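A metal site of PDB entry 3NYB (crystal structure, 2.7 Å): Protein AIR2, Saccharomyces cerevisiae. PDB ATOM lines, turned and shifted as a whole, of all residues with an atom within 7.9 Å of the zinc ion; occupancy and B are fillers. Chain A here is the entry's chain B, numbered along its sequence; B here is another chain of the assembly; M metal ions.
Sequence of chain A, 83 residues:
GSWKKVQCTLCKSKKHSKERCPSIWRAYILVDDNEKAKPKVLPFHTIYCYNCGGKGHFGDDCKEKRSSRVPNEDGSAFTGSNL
The backbone NH of Gly 59 lies close to the side-chain sulfur of Cys 49, at 3.6 Å.
The side-chain sulfur (SG) of Cys 62 lies close to the backbone NH (N) of Glu 64 (3.5 Å).
The side-chain amide oxygen (OD1) of Asn 51 lies close to the side-chain sulfur (SG) of Cys 62.
O of Gly 54 sits at hydrogen-bond distance from N of Cys 49.
The side-chain sulfur (SG) of Cys 52 sits close to the backbone NH (N) of Gly 54 (3.3 Å).
N of Asn 51 sits close to SG of Cys 49, 3.1 Å away.
Four residues have an atom within 4 Å of the zinc ion: Cys 49, Cys 52, His 57 and Cys 62.
The zinc ion is bound by SG of Cys 52 (2.4 Å).
A ring nitrogen (NE2) of His 57 binds the zinc ion, at 2.4 Å.
SG of Cys 62 is bound to the zinc ion (2.4 Å).
The side-chain sulfur (SG) of Cys 49 binds the zinc ion (2.6 Å).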
ATOM      1  N   TYR A  48      23.221  15.877 -25.821  1.00  0.00           N
ATOM      2  CA  TYR A  48      22.487  14.645 -26.044  1.00  0.00           C
ATOM      3  C   TYR A  48      23.403  13.441 -26.125  1.00  0.00           C
ATOM      4  O   TYR A  48      24.454  13.487 -26.750  1.00  0.00           O
ATOM      5  CB  TYR A  48      21.620  14.754 -27.295  1.00  0.00           C
ATOM      6  CG  TYR A  48      20.500  15.752 -27.143  1.00  0.00           C
ATOM      7  CD1 TYR A  48      20.685  17.077 -27.510  1.00  0.00           C
ATOM      8  CD2 TYR A  48      19.270  15.371 -26.644  1.00  0.00           C
ATOM      9  CE1 TYR A  48      19.655  17.997 -27.377  1.00  0.00           C
ATOM     10  CE2 TYR A  48      18.235  16.279 -26.513  1.00  0.00           C
ATOM     11  CZ  TYR A  48      18.442  17.601 -26.881  1.00  0.00           C
ATOM     12  OH  TYR A  48      17.420  18.509 -26.746  1.00  0.00           O
ATOM     13  N   CYS A  49      22.989  12.355 -25.487  1.00  0.00           N
ATOM     14  CA  CYS A  49      23.813  11.165 -25.400  1.00  0.00           C
ATOM     15  C   CYS A  49      23.458  10.157 -26.491  1.00  0.00           C
ATOM     16  O   CYS A  49      22.295   9.832 -26.701  1.00  0.00           O
ATOM     17  CB  CYS A  49      23.647  10.515 -24.032  1.00  0.00           C
ATOM     18  SG  CYS A  49      24.250   8.833 -23.988  1.00  0.00           S
ATOM     19  N   TYR A  50      24.480   9.658 -27.177  1.00  0.00           N
ATOM     20  CA  TYR A  50      24.268   8.767 -28.304  1.00  0.00           C
ATOM     21  C   TYR A  50      23.953   7.356 -27.847  1.00  0.00           C
ATOM     22  O   TYR A  50      23.511   6.522 -28.634  1.00  0.00           O
ATOM     23  CB  TYR A  50      25.479   8.781 -29.236  1.00  0.00           C
ATOM     24  CG  TYR A  50      26.774   8.246 -28.664  1.00  0.00           C
ATOM     25  CD1 TYR A  50      26.879   6.936 -28.205  1.00  0.00           C
ATOM     26  CD2 TYR A  50      27.907   9.047 -28.617  1.00  0.00           C
ATOM     27  CE1 TYR A  50      28.079   6.452 -27.702  1.00  0.00           C
ATOM     28  CE2 TYR A  50      29.108   8.563 -28.114  1.00  0.00           C
ATOM     29  CZ  TYR A  50      29.192   7.272 -27.665  1.00  0.00           C
ATOM     30  OH  TYR A  50      30.386   6.808 -27.168  1.00  0.00           O
ATOM     31  N   ASN A  51      24.160   7.108 -26.565  1.00  0.00           N
ATOM     32  CA  ASN A  51      23.977   5.789 -25.969  1.00  0.00           C
ATOM     33  C   ASN A  51      22.555   5.588 -25.452  1.00  0.00           C
ATOM     34  O   ASN A  51      21.923   4.564 -25.719  1.00  0.00           O
ATOM     35  CB  ASN A  51      24.974   5.583 -24.842  1.00  0.00           C
ATOM     36  CG  ASN A  51      24.970   4.173 -24.313  1.00  0.00           C
ATOM     37  OD1 ASN A  51      25.057   3.948 -23.109  1.00  0.00           O
ATOM     38  ND2 ASN A  51      24.847   3.216 -25.217  1.00  0.00           N
ATOM     39  N   CYS A  52      22.063   6.565 -24.694  1.00  0.00           N
ATOM     40  CA  CYS A  52      20.667   6.642 -24.314  1.00  0.00           C
ATOM     41  C   CYS A  52      20.178   7.982 -24.826  1.00  0.00           C
ATOM     42  O   CYS A  52      20.912   8.968 -24.786  1.00  0.00           O
ATOM     43  CB  CYS A  52      20.522   6.591 -22.791  1.00  0.00           C
ATOM     44  SG  CYS A  52      20.822   8.190 -22.011  1.00  0.00           S
ATOM     45  N   GLY A  53      18.951   8.032 -25.320  1.00  0.00           N
ATOM     46  CA  GLY A  53      18.446   9.261 -25.906  1.00  0.00           C
ATOM     47  C   GLY A  53      18.326  10.388 -24.909  1.00  0.00           C
ATOM     48  O   GLY A  53      17.613  11.358 -25.135  1.00  0.00           O
ATOM     49  N   GLY A  54      19.048  10.271 -23.794  1.00  0.00           N
ATOM     50  CA  GLY A  54      18.957  11.230 -22.701  1.00  0.00           C
ATOM     51  C   GLY A  54      19.759  12.504 -22.895  1.00  0.00           C
ATOM     52  O   GLY A  54      20.796  12.511 -23.568  1.00  0.00           O
ATOM     53  N   LYS A  55      19.280  13.586 -22.292  1.00  0.00           N
ATOM     54  CA  LYS A  55      19.924  14.890 -22.399  1.00  0.00           C
ATOM     55  C   LYS A  55      20.781  15.213 -21.185  1.00  0.00           C
ATOM     56  O   LYS A  55      20.567  14.649 -20.116  1.00  0.00           O
ATOM     57  CB  LYS A  55      18.879  15.991 -22.596  1.00  0.00           C
ATOM     58  CG  LYS A  55      17.897  16.097 -21.459  1.00  0.00           C
ATOM     59  CD  LYS A  55      16.494  16.449 -21.944  1.00  0.00           C
ATOM     60  CE  LYS A  55      16.486  17.722 -22.771  1.00  0.00           C
ATOM     61  NZ  LYS A  55      15.105  18.059 -23.198  1.00  0.00           N
ATOM     62  N   HIS A  57      24.258  15.005 -21.087  1.00  0.00           N
ATOM     63  CA  HIS A  57      25.570  14.376 -21.113  1.00  0.00           C
ATOM     64  C   HIS A  57      25.858  13.696 -22.452  1.00  0.00           C
ATOM     65  O   HIS A  57      24.922  13.356 -23.190  1.00  0.00           O
ATOM     66  CB  HIS A  57      25.686  13.339 -19.985  1.00  0.00           C
ATOM     67  CG  HIS A  57      24.800  12.153 -20.173  1.00  0.00           C
ATOM     68  ND1 HIS A  57      23.447  12.174 -19.882  1.00  0.00           N
ATOM     69  CD2 HIS A  57      25.073  10.899 -20.606  1.00  0.00           C
ATOM     70  CE1 HIS A  57      22.934  10.991 -20.143  1.00  0.00           C
ATOM     71  NE2 HIS A  57      23.888  10.196 -20.592  1.00  0.00           N
ATOM     72  N   PHE A  58      27.131  13.510 -22.761  1.00  0.00           N
ATOM     73  CA  PHE A  58      27.529  12.853 -24.002  1.00  0.00           C
ATOM     74  C   PHE A  58      27.421  11.338 -23.949  1.00  0.00           C
ATOM     75  O   PHE A  58      27.625  10.727 -22.891  1.00  0.00           O
ATOM     76  CB  PHE A  58      28.959  13.242 -24.374  1.00  0.00           C
ATOM     77  CG  PHE A  58      29.109  14.668 -24.771  1.00  0.00           C
ATOM     78  CD1 PHE A  58      28.363  15.201 -25.814  1.00  0.00           C
ATOM     79  CD2 PHE A  58      30.008  15.496 -24.119  1.00  0.00           C
ATOM     80  CE1 PHE A  58      28.497  16.517 -26.183  1.00  0.00           C
ATOM     81  CE2 PHE A  58      30.156  16.813 -24.485  1.00  0.00           C
ATOM     82  CZ  PHE A  58      29.390  17.324 -25.529  1.00  0.00           C
ATOM     83  N   GLY A  59      27.111  10.731 -25.082  1.00  0.00           N
ATOM     84  CA  GLY A  59      26.973   9.284 -25.175  1.00  0.00           C
ATOM     85  C   GLY A  59      28.211   8.510 -24.766  1.00  0.00           C
ATOM     86  O   GLY A  59      28.147   7.319 -24.468  1.00  0.00           O
ATOM     87  N   ASP A  60      29.341   9.196 -24.736  1.00  0.00           N
ATOM     88  CA  ASP A  60      30.602   8.527 -24.461  1.00  0.00           C
ATOM     89  C   ASP A  60      30.796   8.264 -22.968  1.00  0.00           C
ATOM     90  O   ASP A  60      31.214   7.172 -22.579  1.00  0.00           O
ATOM     91  CB  ASP A  60      31.757   9.365 -25.006  1.00  0.00           C
ATOM     92  CG  ASP A  60      32.867   8.528 -25.560  1.00  0.00           C
ATOM     93  OD1 ASP A  60      33.711   8.054 -24.780  1.00  0.00           O
ATOM     94  OD2 ASP A  60      32.895   8.332 -26.788  1.00  0.00           O
ATOM     95  N   ASP A  61      30.495   9.264 -22.138  1.00  0.00           N
ATOM     96  CA  ASP A  61      30.638   9.123 -20.702  1.00  0.00           C
ATOM     97  C   ASP A  61      29.284   8.966 -20.019  1.00  0.00           C
ATOM     98  O   ASP A  61      28.941   9.676 -19.076  1.00  0.00           O
ATOM     99  CB  ASP A  61      31.436  10.296 -20.112  1.00  0.00           C
ATOM    100  CG  ASP A  61      31.132  11.616 -20.786  1.00  0.00           C
ATOM    101  OD1 ASP A  61      32.100  12.290 -21.203  1.00  0.00           O
ATOM    102  OD2 ASP A  61      29.946  11.982 -20.912  1.00  0.00           O
ATOM    103  N   CYS A  62      28.508   8.012 -20.528  1.00  0.00           N
ATOM    104  CA  CYS A  62      27.160   7.755 -20.056  1.00  0.00           C
ATOM    105  C   CYS A  62      27.148   6.574 -19.096  1.00  0.00           C
ATOM    106  O   CYS A  62      28.092   5.772 -19.080  1.00  0.00           O
ATOM    107  CB  CYS A  62      26.246   7.538 -21.276  1.00  0.00           C
ATOM    108  SG  CYS A  62      24.819   6.479 -21.077  1.00  0.00           S
ATOM    109  N   LYS A  63      26.101   6.462 -18.284  1.00  0.00           N
ATOM    110  CA  LYS A  63      26.083   5.485 -17.193  1.00  0.00           C
ATOM    111  C   LYS A  63      25.510   4.116 -17.564  1.00  0.00           C
ATOM    112  O   LYS A  63      25.872   3.109 -16.962  1.00  0.00           O
ATOM    113  CB  LYS A  63      25.324   6.045 -15.980  1.00  0.00           C
ATOM    114  CG  LYS A  63      25.825   7.407 -15.532  1.00  0.00           C
ATOM    115  CD  LYS A  63      27.340   7.441 -15.462  1.00  0.00           C
ATOM    116  CE  LYS A  63      27.854   8.854 -15.205  1.00  0.00           C
ATOM    117  NZ  LYS A  63      29.320   8.972 -15.459  1.00  0.00           N
ATOM    118  N   GLU A  64      24.605   4.098 -18.543  1.00  0.00           N
ATOM    119  CA  GLU A  64      23.924   2.868 -18.931  1.00  0.00           C
ATOM    120  C   GLU A  64      24.837   1.878 -19.642  1.00  0.00           C
ATOM    121  O   GLU A  64      25.913   2.245 -20.112  1.00  0.00           O
ATOM    122  CB  GLU A  64      22.741   3.208 -19.838  1.00  0.00           C
ATOM    123  CG  GLU A  64      21.847   4.323 -19.309  1.00  0.00           C
ATOM    124  CD  GLU A  64      20.830   3.823 -18.301  1.00  0.00           C
ATOM    125  OE1 GLU A  64      20.092   2.869 -18.627  1.00  0.00           O
ATOM    126  OE2 GLU A  64      20.759   4.397 -17.189  1.00  0.00           O
ATOM    127  N   LYS A  65      24.416   0.613 -19.712  1.00  0.00           N
ATOM    128  CA  LYS A  65      25.110  -0.364 -20.535  1.00  0.00           C
ATOM    129  C   LYS A  65      25.093   0.168 -21.957  1.00  0.00           C
ATOM    130  O   LYS A  65      24.079   0.713 -22.404  1.00  0.00           O
ATOM    131  CB  LYS A  65      24.407  -1.722 -20.491  1.00  0.00           C
ATOM    132  CG  LYS A  65      24.624  -2.527 -19.225  1.00  0.00           C
ATOM    133  CD  LYS A  65      24.320  -3.993 -19.460  1.00  0.00           C
ATOM    134  CE  LYS A  65      24.284  -4.776 -18.159  1.00  0.00           C
ATOM    135  NZ  LYS A  65      23.110  -4.416 -17.316  1.00  0.00           N
ATOM    136  N   VAL B 234      18.442   4.926 -29.519  1.00  0.00           N
ATOM    137  CA  VAL B 234      18.398   6.374 -29.751  1.00  0.00           C
ATOM    138  C   VAL B 234      17.770   6.772 -31.086  1.00  0.00           C
ATOM    139  O   VAL B 234      18.055   6.170 -32.113  1.00  0.00           O
ATOM    140  CB  VAL B 234      19.805   6.994 -29.671  1.00  0.00           C
ATOM    141  CG1 VAL B 234      19.725   8.511 -29.733  1.00  0.00           C
ATOM    142  CG2 VAL B 234      20.500   6.549 -28.406  1.00  0.00           C
HETATM  143 ZN    ZN M   1      23.159   8.156 -21.683  1.00  0.00          ZN
